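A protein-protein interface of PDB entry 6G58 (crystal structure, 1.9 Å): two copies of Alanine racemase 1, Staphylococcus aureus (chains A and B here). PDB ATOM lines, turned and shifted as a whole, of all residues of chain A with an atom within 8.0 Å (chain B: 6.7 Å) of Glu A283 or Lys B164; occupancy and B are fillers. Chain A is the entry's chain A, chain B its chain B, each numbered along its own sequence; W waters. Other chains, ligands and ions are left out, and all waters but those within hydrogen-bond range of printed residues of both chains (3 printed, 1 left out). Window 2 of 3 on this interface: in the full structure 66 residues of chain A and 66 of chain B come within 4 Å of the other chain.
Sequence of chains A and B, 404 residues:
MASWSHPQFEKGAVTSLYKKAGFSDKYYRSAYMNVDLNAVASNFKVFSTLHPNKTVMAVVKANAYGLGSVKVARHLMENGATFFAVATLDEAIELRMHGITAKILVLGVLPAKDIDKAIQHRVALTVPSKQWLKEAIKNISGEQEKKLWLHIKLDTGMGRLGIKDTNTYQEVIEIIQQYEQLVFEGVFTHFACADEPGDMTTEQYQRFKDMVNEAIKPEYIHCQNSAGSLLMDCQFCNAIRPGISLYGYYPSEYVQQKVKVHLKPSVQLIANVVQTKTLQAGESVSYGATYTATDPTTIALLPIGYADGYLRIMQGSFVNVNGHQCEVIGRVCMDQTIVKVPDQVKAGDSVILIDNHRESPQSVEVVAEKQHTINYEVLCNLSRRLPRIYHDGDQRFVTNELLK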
ATOM      1  N   LYS A 277      -5.246   8.902 -21.560  1.00  0.00           N
ATOM      2  CA  LYS A 277      -5.388  10.332 -21.807  1.00  0.00           C
ATOM      3  C   LYS A 277      -6.819  10.767 -21.445  1.00  0.00           C
ATOM      4  O   LYS A 277      -7.738   9.965 -21.527  1.00  0.00           O
ATOM      5  CB  LYS A 277      -5.117  10.579 -23.290  1.00  0.00           C
ATOM      6  CG  LYS A 277      -5.225  12.034 -23.680  1.00  0.00           C
ATOM      7  CD  LYS A 277      -4.851  12.280 -25.116  1.00  0.00           C
ATOM      8  CE  LYS A 277      -6.012  12.041 -26.065  1.00  0.00           C
ATOM      9  NZ  LYS A 277      -6.305  13.291 -26.813  1.00  0.00           N
ATOM     10  N   THR A 278      -7.014  12.022 -21.064  1.00  0.00           N
ATOM     11  CA  THR A 278      -8.343  12.554 -20.720  1.00  0.00           C
ATOM     12  C   THR A 278      -8.842  13.456 -21.827  1.00  0.00           C
ATOM     13  O   THR A 278      -8.213  14.459 -22.120  1.00  0.00           O
ATOM     14  CB  THR A 278      -8.286  13.354 -19.422  1.00  0.00           C
ATOM     15  OG1 THR A 278      -7.901  12.478 -18.364  1.00  0.00           O
ATOM     16  CG2 THR A 278      -9.638  13.962 -19.081  1.00  0.00           C
ATOM     17  N   LEU A 279      -9.961  13.100 -22.450  1.00  0.00           N
ATOM     18  CA  LEU A 279     -10.660  14.022 -23.364  1.00  0.00           C
ATOM     19  C   LEU A 279     -11.588  14.873 -22.561  1.00  0.00           C
ATOM     20  O   LEU A 279     -12.283  14.355 -21.705  1.00  0.00           O
ATOM     21  CB  LEU A 279     -11.561  13.290 -24.341  1.00  0.00           C
ATOM     22  CG  LEU A 279     -11.018  12.341 -25.356  1.00  0.00           C
ATOM     23  CD1 LEU A 279     -12.208  11.668 -26.032  1.00  0.00           C
ATOM     24  CD2 LEU A 279     -10.128  13.070 -26.345  1.00  0.00           C
ATOM     25  N   GLN A 280     -11.637  16.151 -22.879  1.00  0.00           N
ATOM     26  CA  GLN A 280     -12.635  17.050 -22.326  1.00  0.00           C
ATOM     27  C   GLN A 280     -13.837  17.105 -23.267  1.00  0.00           C
ATOM     28  O   GLN A 280     -13.739  16.739 -24.451  1.00  0.00           O
ATOM     29  CB  GLN A 280     -12.048  18.462 -22.129  1.00  0.00           C
ATOM     30  CG  GLN A 280     -10.927  18.547 -21.088  1.00  0.00           C
ATOM     31  CD  GLN A 280     -11.355  18.047 -19.715  1.00  0.00           C
ATOM     32  OE1 GLN A 280     -12.501  18.273 -19.277  1.00  0.00           O
ATOM     33  NE2 GLN A 280     -10.445  17.345 -19.039  1.00  0.00           N
ATOM     34  N   ALA A 281     -14.969  17.541 -22.720  1.00  0.00           N
ATOM     35  CA  ALA A 281     -16.197  17.759 -23.483  1.00  0.00           C
ATOM     36  C   ALA A 281     -15.906  18.560 -24.759  1.00  0.00           C
ATOM     37  O   ALA A 281     -15.209  19.580 -24.704  1.00  0.00           O
ATOM     38  CB  ALA A 281     -17.226  18.504 -22.621  1.00  0.00           C
ATOM     39  N   GLY A 282     -16.418  18.083 -25.898  1.00  0.00           N
ATOM     40  CA  GLY A 282     -16.206  18.754 -27.186  1.00  0.00           C
ATOM     41  C   GLY A 282     -14.963  18.296 -27.949  1.00  0.00           C
ATOM     42  O   GLY A 282     -14.787  18.668 -29.105  1.00  0.00           O
ATOM     43  N   GLU A 283     -14.101  17.491 -27.335  1.00  0.00           N
ATOM     44  CA  GLU A 283     -12.937  16.960 -28.054  1.00  0.00           C
ATOM     45  C   GLU A 283     -13.279  15.636 -28.699  1.00  0.00           C
ATOM     46  O   GLU A 283     -13.921  14.777 -28.079  1.00  0.00           O
ATOM     47  CB  GLU A 283     -11.738  16.786 -27.133  1.00  0.00           C
ATOM     48  CG  GLU A 283     -11.317  18.104 -26.504  1.00  0.00           C
ATOM     49  CD  GLU A 283     -10.011  17.993 -25.771  1.00  0.00           C
ATOM     50  OE1 GLU A 283      -9.775  16.949 -25.103  1.00  0.00           O
ATOM     51  OE2 GLU A 283      -9.231  18.957 -25.875  1.00  0.00           O
ATOM     52  N   SER A 284     -12.823  15.481 -29.934  1.00  0.00           N
ATOM     53  CA  SER A 284     -13.091  14.292 -30.722  1.00  0.00           C
ATOM     54  C   SER A 284     -11.891  13.356 -30.753  1.00  0.00           C
ATOM     55  O   SER A 284     -10.815  13.695 -30.288  1.00  0.00           O
ATOM     56  CB  SER A 284     -13.517  14.708 -32.139  1.00  0.00           C
ATOM     57  OG  SER A 284     -12.398  15.184 -32.882  1.00  0.00           O
ATOM     58  N   VAL A 285     -12.091  12.164 -31.278  1.00  0.00           N
ATOM     59  CA  VAL A 285     -11.017  11.218 -31.406  1.00  0.00           C
ATOM     60  C   VAL A 285     -11.054  10.484 -32.743  1.00  0.00           C
ATOM     61  O   VAL A 285     -12.117  10.022 -33.226  1.00  0.00           O
ATOM     62  CB  VAL A 285     -10.945  10.207 -30.224  1.00  0.00           C
ATOM     63  CG1 VAL A 285     -10.638  10.891 -28.910  1.00  0.00           C
ATOM     64  CG2 VAL A 285     -12.233   9.432 -30.078  1.00  0.00           C
ATOM     65  N   SER A 286      -9.847  10.361 -33.312  1.00  0.00           N
ATOM     66  CA  SER A 286      -9.543   9.552 -34.472  1.00  0.00           C
ATOM     67  C   SER A 286     -10.109  10.153 -35.801  1.00  0.00           C
ATOM     68  O   SER A 286     -10.642  11.268 -35.830  1.00  0.00           O
ATOM     69  CB  SER A 286      -9.980   8.111 -34.236  1.00  0.00           C
ATOM     70  OG  SER A 286      -9.398   7.267 -35.177  1.00  0.00           O
ATOM     71  N   ALA A 289     -13.432  12.430 -36.819  1.00  0.00           N
ATOM     72  CA  ALA A 289     -14.005  13.003 -35.584  1.00  0.00           C
ATOM     73  C   ALA A 289     -15.383  12.351 -35.286  1.00  0.00           C
ATOM     74  O   ALA A 289     -16.350  12.992 -35.022  1.00  0.00           O
ATOM     75  CB  ALA A 289     -14.135  14.515 -35.708  1.00  0.00           C
ATOM     76  N   TYR A 291     -16.257  10.228 -32.885  1.00  0.00           N
ATOM     77  CA  TYR A 291     -16.622  10.213 -31.463  1.00  0.00           C
ATOM     78  C   TYR A 291     -16.196  11.539 -30.878  1.00  0.00           C
ATOM     79  O   TYR A 291     -15.056  11.961 -31.061  1.00  0.00           O
ATOM     80  CB  TYR A 291     -15.911   9.085 -30.701  1.00  0.00           C
ATOM     81  CG  TYR A 291     -16.262   9.041 -29.228  1.00  0.00           C
ATOM     82  CD1 TYR A 291     -15.588   9.828 -28.306  1.00  0.00           C
ATOM     83  CD2 TYR A 291     -17.315   8.218 -28.755  1.00  0.00           C
ATOM     84  CE1 TYR A 291     -15.943   9.825 -26.965  1.00  0.00           C
ATOM     85  CE2 TYR A 291     -17.671   8.203 -27.410  1.00  0.00           C
ATOM     86  CZ  TYR A 291     -16.978   9.014 -26.522  1.00  0.00           C
ATOM     87  OH  TYR A 291     -17.282   9.010 -25.195  1.00  0.00           O
ATOM     88  N   THR A 292     -17.123  12.185 -30.179  1.00  0.00           N
ATOM     89  CA  THR A 292     -16.874  13.438 -29.468  1.00  0.00           C
ATOM     90  C   THR A 292     -17.319  13.227 -28.020  1.00  0.00           C
ATOM     91  O   THR A 292     -18.419  12.752 -27.780  1.00  0.00           O
ATOM     92  CB  THR A 292     -17.645  14.614 -30.113  1.00  0.00           C
ATOM     93  OG1 THR A 292     -17.293  14.696 -31.495  1.00  0.00           O
ATOM     94  CG2 THR A 292     -17.306  15.950 -29.433  1.00  0.00           C
ATOM     95  N   ALA A 293     -16.455  13.558 -27.071  1.00  0.00           N
ATOM     96  CA  ALA A 293     -16.795  13.462 -25.650  1.00  0.00           C
ATOM     97  C   ALA A 293     -17.853  14.504 -25.266  1.00  0.00           C
ATOM     98  O   ALA A 293     -17.772  15.679 -25.660  1.00  0.00           O
ATOM     99  CB  ALA A 293     -15.559  13.614 -24.777  1.00  0.00           C
ATOM    100  N   THR A 294     -18.843  14.049 -24.501  1.00  0.00           N
ATOM    101  CA  THR A 294     -19.875  14.916 -23.914  1.00  0.00           C
ATOM    102  C   THR A 294     -19.434  15.443 -22.533  1.00  0.00           C
ATOM    103  O   THR A 294     -19.727  16.587 -22.202  1.00  0.00           O
ATOM    104  CB  THR A 294     -21.228  14.169 -23.817  1.00  0.00           C
ATOM    105  OG1 THR A 294     -21.067  12.968 -23.048  1.00  0.00           O
ATOM    106  CG2 THR A 294     -21.731  13.778 -25.216  1.00  0.00           C
ATOM    107  N   ASP A 295     -18.725  14.616 -21.752  1.00  0.00           N
ATOM    108  CA  ASP A 295     -18.103  15.027 -20.466  1.00  0.00           C
ATOM    109  C   ASP A 295     -16.702  14.393 -20.322  1.00  0.00           C
ATOM    110  O   ASP A 295     -16.335  13.556 -21.149  1.00  0.00           O
ATOM    111  CB  ASP A 295     -19.013  14.686 -19.260  1.00  0.00           C
ATOM    112  CG  ASP A 295     -19.800  13.409 -19.452  1.00  0.00           C
ATOM    113  OD1 ASP A 295     -19.277  12.467 -20.070  1.00  0.00           O
ATOM    114  OD2 ASP A 295     -20.954  13.354 -18.981  1.00  0.00           O
ATOM    115  N   THR A 297     -13.723  12.234 -20.162  1.00  0.00           N
ATOM    116  CA  THR A 297     -13.682  10.838 -20.525  1.00  0.00           C
ATOM    117  C   THR A 297     -12.214  10.412 -20.580  1.00  0.00           C
ATOM    118  O   THR A 297     -11.427  11.045 -21.278  1.00  0.00           O
ATOM    119  CB  THR A 297     -14.318  10.661 -21.933  1.00  0.00           C
ATOM    120  OG1 THR A 297     -15.660  11.172 -21.946  1.00  0.00           O
ATOM    121  CG2 THR A 297     -14.319   9.228 -22.365  1.00  0.00           C
ATOM    122  N   ILE A 299      -9.491   7.877 -22.019  1.00  0.00           N
ATOM    123  CA  ILE A 299      -9.296   6.959 -23.128  1.00  0.00           C
ATOM    124  C   ILE A 299      -7.925   6.271 -23.027  1.00  0.00           C
ATOM    125  O   ILE A 299      -7.018   6.763 -22.356  1.00  0.00           O
ATOM    126  CB  ILE A 299      -9.480   7.634 -24.501  1.00  0.00           C
ATOM    127  CG1 ILE A 299      -8.394   8.692 -24.757  1.00  0.00           C
ATOM    128  CG2 ILE A 299     -10.861   8.266 -24.592  1.00  0.00           C
ATOM    129  CD1 ILE A 299      -8.417   9.222 -26.182  1.00  0.00           C
ATOM    130  N   PRO B 128       5.814  10.715 -27.517  1.00  0.00           N
ATOM    131  CA  PRO B 128       4.411  11.045 -27.347  1.00  0.00           C
ATOM    132  C   PRO B 128       4.076  11.880 -26.133  1.00  0.00           C
ATOM    133  O   PRO B 128       2.952  12.396 -26.047  1.00  0.00           O
ATOM    134  CB  PRO B 128       3.760   9.665 -27.200  1.00  0.00           C
ATOM    135  CG  PRO B 128       4.795   8.876 -26.467  1.00  0.00           C
ATOM    136  CD  PRO B 128       6.112   9.360 -27.034  1.00  0.00           C
ATOM    137  N   LYS B 153       5.800  14.272 -31.212  1.00  0.00           N
ATOM    138  CA  LYS B 153       4.473  14.254 -31.781  1.00  0.00           C
ATOM    139  C   LYS B 153       3.552  15.166 -30.999  1.00  0.00           C
ATOM    140  O   LYS B 153       3.382  15.001 -29.778  1.00  0.00           O
ATOM    141  CB  LYS B 153       3.897  12.832 -31.734  1.00  0.00           C
ATOM    142  CG  LYS B 153       2.538  12.656 -32.388  1.00  0.00           C
ATOM    143  CD  LYS B 153       2.038  11.252 -32.023  1.00  0.00           C
ATOM    144  CE  LYS B 153       0.769  10.887 -32.751  1.00  0.00           C
ATOM    145  NZ  LYS B 153       0.134   9.625 -32.184  1.00  0.00           N
ATOM    146  N   LEU B 154       2.923  16.097 -31.713  1.00  0.00           N
ATOM    147  CA  LEU B 154       1.886  16.981 -31.176  1.00  0.00           C
ATOM    148  C   LEU B 154       0.492  16.507 -31.580  1.00  0.00           C
ATOM    149  O   LEU B 154       0.248  16.129 -32.745  1.00  0.00           O
ATOM    150  CB  LEU B 154       2.107  18.432 -31.635  1.00  0.00           C
ATOM    151  CG  LEU B 154       3.516  18.992 -31.404  1.00  0.00           C
ATOM    152  CD1 LEU B 154       3.662  20.445 -31.800  1.00  0.00           C
ATOM    153  CD2 LEU B 154       3.943  18.823 -29.951  1.00  0.00           C
ATOM    154  N   ASP B 155      -0.439  16.567 -30.632  1.00  0.00           N
ATOM    155  CA  ASP B 155      -1.838  16.300 -30.878  1.00  0.00           C
ATOM    156  C   ASP B 155      -2.486  17.680 -31.043  1.00  0.00           C
ATOM    157  O   ASP B 155      -2.570  18.476 -30.094  1.00  0.00           O
ATOM    158  CB  ASP B 155      -2.442  15.514 -29.707  1.00  0.00           C
ATOM    159  CG  ASP B 155      -3.977  15.382 -29.775  1.00  0.00           C
ATOM    160  OD1 ASP B 155      -4.585  15.630 -30.827  1.00  0.00           O
ATOM    161  OD2 ASP B 155      -4.587  14.990 -28.739  1.00  0.00           O
ATOM    162  N   THR B 156      -2.922  17.938 -32.275  1.00  0.00           N
ATOM    163  CA  THR B 156      -3.634  19.129 -32.639  1.00  0.00           C
ATOM    164  C   THR B 156      -5.107  18.858 -32.962  1.00  0.00           C
ATOM    165  O   THR B 156      -5.768  19.727 -33.489  1.00  0.00           O
ATOM    166  CB  THR B 156      -2.971  19.823 -33.814  1.00  0.00           C
ATOM    167  OG1 THR B 156      -2.940  18.941 -34.956  1.00  0.00           O
ATOM    168  CG2 THR B 156      -1.555  20.260 -33.429  1.00  0.00           C
ATOM    169  N   GLY B 157      -5.618  17.664 -32.645  1.00  0.00           N
ATOM    170  CA  GLY B 157      -7.041  17.318 -32.896  1.00  0.00           C
ATOM    171  C   GLY B 157      -7.342  15.862 -33.211  1.00  0.00           C
ATOM    172  O   GLY B 157      -8.488  15.425 -33.116  1.00  0.00           O
ATOM    173  N   GLY B 159      -6.504  13.373 -31.429  1.00  0.00           N
ATOM    174  CA  GLY B 159      -6.918  12.855 -30.147  1.00  0.00           C
ATOM    175  C   GLY B 159      -6.386  11.452 -29.830  1.00  0.00           C
ATOM    176  O   GLY B 159      -7.006  10.709 -29.077  1.00  0.00           O
ATOM    177  N   ARG B 160      -5.255  11.073 -30.417  1.00  0.00           N
ATOM    178  CA  ARG B 160      -4.606   9.813 -30.011  1.00  0.00           C
ATOM    179  C   ARG B 160      -3.477  10.218 -29.047  1.00  0.00           C
ATOM    180  O   ARG B 160      -3.645  11.163 -28.263  1.00  0.00           O
ATOM    181  CB  ARG B 160      -4.160   9.005 -31.247  1.00  0.00           C
ATOM    182  CG  ARG B 160      -5.350   8.605 -32.114  1.00  0.00           C
ATOM    183  CD  ARG B 160      -4.965   7.705 -33.285  1.00  0.00           C
ATOM    184  NE  ARG B 160      -3.900   8.295 -34.120  1.00  0.00           N
ATOM    185  CZ  ARG B 160      -3.370   7.719 -35.210  1.00  0.00           C
ATOM    186  NH1 ARG B 160      -3.771   6.524 -35.636  1.00  0.00           N
ATOM    187  NH2 ARG B 160      -2.405   8.336 -35.884  1.00  0.00           N
ATOM    188  N   GLY B 162      -0.079  12.149 -28.077  1.00  0.00           N
ATOM    189  CA  GLY B 162       0.680  13.285 -28.524  1.00  0.00           C
ATOM    190  C   GLY B 162       0.509  14.382 -27.501  1.00  0.00           C
ATOM    191  O   GLY B 162      -0.504  14.430 -26.764  1.00  0.00           O
ATOM    192  N   ILE B 163       1.449  15.306 -27.552  1.00  0.00           N
ATOM    193  CA  ILE B 163       1.501  16.409 -26.632  1.00  0.00           C
ATOM    194  C   ILE B 163       0.506  17.483 -27.120  1.00  0.00           C
ATOM    195  O   ILE B 163       0.559  17.886 -28.285  1.00  0.00           O
ATOM    196  CB  ILE B 163       2.944  16.944 -26.572  1.00  0.00           C
ATOM    197  CG1 ILE B 163       3.847  15.898 -25.919  1.00  0.00           C
ATOM    198  CG2 ILE B 163       3.013  18.300 -25.869  1.00  0.00           C
ATOM    199  CD1 ILE B 163       5.307  16.033 -26.249  1.00  0.00           C
ATOM    200  N   LYS B 164      -0.354  17.937 -26.236  1.00  0.00           N
ATOM    201  CA  LYS B 164      -1.359  18.907 -26.572  1.00  0.00           C
ATOM    202  C   LYS B 164      -1.028  20.329 -26.187  1.00  0.00           C
ATOM    203  O   LYS B 164      -1.600  21.261 -26.751  1.00  0.00           O
ATOM    204  CB  LYS B 164      -2.626  18.622 -25.812  1.00  0.00           C
ATOM    205  CG  LYS B 164      -3.275  17.340 -26.227  1.00  0.00           C
ATOM    206  CD  LYS B 164      -4.663  17.223 -25.617  1.00  0.00           C
ATOM    207  CE  LYS B 164      -5.578  18.259 -26.245  1.00  0.00           C
ATOM    208  NZ  LYS B 164      -6.966  17.868 -25.983  1.00  0.00           N
ATOM    209  N   ASP B 165      -0.172  20.491 -25.192  1.00  0.00           N
ATOM    210  CA  ASP B 165       0.113  21.828 -24.679  1.00  0.00           C
ATOM    211  C   ASP B 165       1.542  22.262 -24.958  1.00  0.00           C
ATOM    212  O   ASP B 165       2.502  21.456 -24.943  1.00  0.00           O
ATOM    213  CB  ASP B 165      -0.244  21.908 -23.200  1.00  0.00           C
ATOM    214  CG  ASP B 165       0.754  21.222 -22.347  1.00  0.00           C
ATOM    215  OD1 ASP B 165       0.770  19.962 -22.353  1.00  0.00           O
ATOM    216  OD2 ASP B 165       1.549  21.945 -21.713  1.00  0.00           O
ATOM    217  N   THR B 166       1.688  23.549 -25.227  1.00  0.00           N
ATOM    218  CA  THR B 166       2.960  24.124 -25.588  1.00  0.00           C
ATOM    219  C   THR B 166       4.028  23.994 -24.513  1.00  0.00           C
ATOM    220  O   THR B 166       5.177  23.710 -24.849  1.00  0.00           O
ATOM    221  CB  THR B 166       2.748  25.618 -25.982  1.00  0.00           C
ATOM    222  OG1 THR B 166       1.881  25.628 -27.102  1.00  0.00           O
ATOM    223  CG2 THR B 166       4.031  26.270 -26.392  1.00  0.00           C
ATOM    224  N   THR B 168       4.478  21.616 -22.283  1.00  0.00           N
ATOM    225  CA  THR B 168       5.015  20.262 -22.341  1.00  0.00           C
ATOM    226  C   THR B 168       5.995  20.099 -23.528  1.00  0.00           C
ATOM    227  O   THR B 168       7.062  19.501 -23.386  1.00  0.00           O
ATOM    228  CB  THR B 168       3.876  19.230 -22.440  1.00  0.00           C
ATOM    229  OG1 THR B 168       3.053  19.307 -21.270  1.00  0.00           O
ATOM    230  CG2 THR B 168       4.464  17.828 -22.557  1.00  0.00           C
ATOM    231  N   ARG B 207      -2.814  25.547 -35.339  1.00  0.00           N
ATOM    232  CA  ARG B 207      -2.432  25.154 -33.974  1.00  0.00           C
ATOM    233  C   ARG B 207      -1.007  24.586 -33.948  1.00  0.00           C
ATOM    234  O   ARG B 207      -0.232  24.881 -33.036  1.00  0.00           O
ATOM    235  CB  ARG B 207      -3.463  24.180 -33.394  1.00  0.00           C
ATOM    236  CG  ARG B 207      -3.097  23.545 -32.075  1.00  0.00           C
ATOM    237  CD  ARG B 207      -3.036  24.567 -30.979  1.00  0.00           C
ATOM    238  NE  ARG B 207      -2.493  23.979 -29.746  1.00  0.00           N
ATOM    239  CZ  ARG B 207      -1.988  24.699 -28.731  1.00  0.00           C
ATOM    240  NH1 ARG B 207      -1.905  26.024 -28.801  1.00  0.00           N
ATOM    241  NH2 ARG B 207      -1.572  24.084 -27.643  1.00  0.00           N
ATOM    242  N   MET B 211       2.246  26.158 -31.830  1.00  0.00           N
ATOM    243  CA  MET B 211       3.088  25.430 -30.869  1.00  0.00           C
ATOM    244  C   MET B 211       4.540  25.445 -31.321  1.00  0.00           C
ATOM    245  O   MET B 211       5.426  25.778 -30.541  1.00  0.00           O
ATOM    246  CB  MET B 211       2.594  23.977 -30.718  1.00  0.00           C
ATOM    247  CG  MET B 211       1.179  23.886 -30.177  1.00  0.00           C
ATOM    248  SD  MET B 211       0.548  22.195 -30.069  1.00  0.00           S
ATOM    249  CE  MET B 211       1.445  21.632 -28.654  1.00  0.00           C
HETATM  250  O   HOH W   1     -10.611  13.554 -34.094  1.00  0.00           O
HETATM  251  O   HOH W   2      -9.157  15.694 -30.360  1.00  0.00           O
HETATM  252  O   HOH W   3      -7.100  15.844 -28.438  1.00  0.00           O
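The side-chain amino group (NZ) of Lys A277 is in salt-bridge range of the side-chain carboxylate (OD2) of Asp B155 (3.1 Å). The side-chain carboxylate (OE2) of Glu A283 is in salt-bridge range of the side-chain amino group (NZ) of Lys B164, 2.5 Å away.
The backbone carbonyl oxygen of Lys B164 lies within hydrogen-bond range of the guanidinium group of Arg B207 (3.0 Å). The backbone NH (N) of Asp B155 sits at hydrogen-bond distance from the backbone carbonyl oxygen (O) of Ile B163 (2.9 Å). The side-chain carboxylate (OE1) of Glu A283 is in hydrogen-bond range of the backbone NH (N) of Gln A280, at 3.0 Å. N of Val A285 is in hydrogen-bond range of O of Tyr A291, 3.0 Å away. The backbone NH of Ala A293 sits at hydrogen-bond distance from the backbone carbonyl oxygen of Glu A283, 3.0 Å away. The backbone NH (N) of Gly B157 sits at hydrogen-bond distance from the side-chain carboxylate (OD1) of Asp B155, 2.9 Å away.
CA of Gly B159 touches NZ of Lys A277, at 3.4 Å. Lys A277 touches Arg B160 (CE to O, 3.3 Å). Ser A284 touches Gly B157 (OG to O, 3.9 Å). Ser A284 touches Gly B159 (O to CA, 3.99 Å). Gly B159 touches Val A285. Gly B159 touches Ile A299.
Of the printed residues of chain B, Glu A283 touches Lys B164 (2.5 Å). Printed residues of chain A within 4 Å of Asp B155: Lys A277. Of the printed residues of chain A, Gly B157 touches Ser A284 (3.9 Å). Of the printed residues of chain A, Arg B160 touches Lys A277 (3.3 Å). Lys B164 touches just one residue of chain A: Glu A283. The nearest residue of chain B that does not touch Glu A283 is Gly B157 (6.5 Å). The nearest residue of chain A that does not touch Lys B164 is Lys A277 (4.4 Å).
Printed residues of chain B that touch a printed residue of chain A: Asp B155, Gly B157, Gly B159, Arg B160 and Lys B164. Printed residues of chain A that touch a printed residue of chain B: Lys A277, Glu A283, Ser A284, Val A285 and Ile A299. Among the printed residues, 8 pairs touch across the chains.
No position is printed for both chains. Of the 8 pairs that touch across the chains among the printed residues, none has its exchanged pair printed and touching as well.
Water W2 bridges O of Ser A284 and O of Gly B157. Water W3 lies within hydrogen-bond range of OD2 of Asp B155 (2.7 Å), NZ of Lys A277 (3.1 Å) and NZ of Lys B164 (3.2 Å). Water W1 lies within hydrogen-bond range of OG of Ser A284 (2.7 Å), O of Ser A286 (2.9 Å), O of Gly B157 (3.0 Å) and N of Val A285 (3.5 Å).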
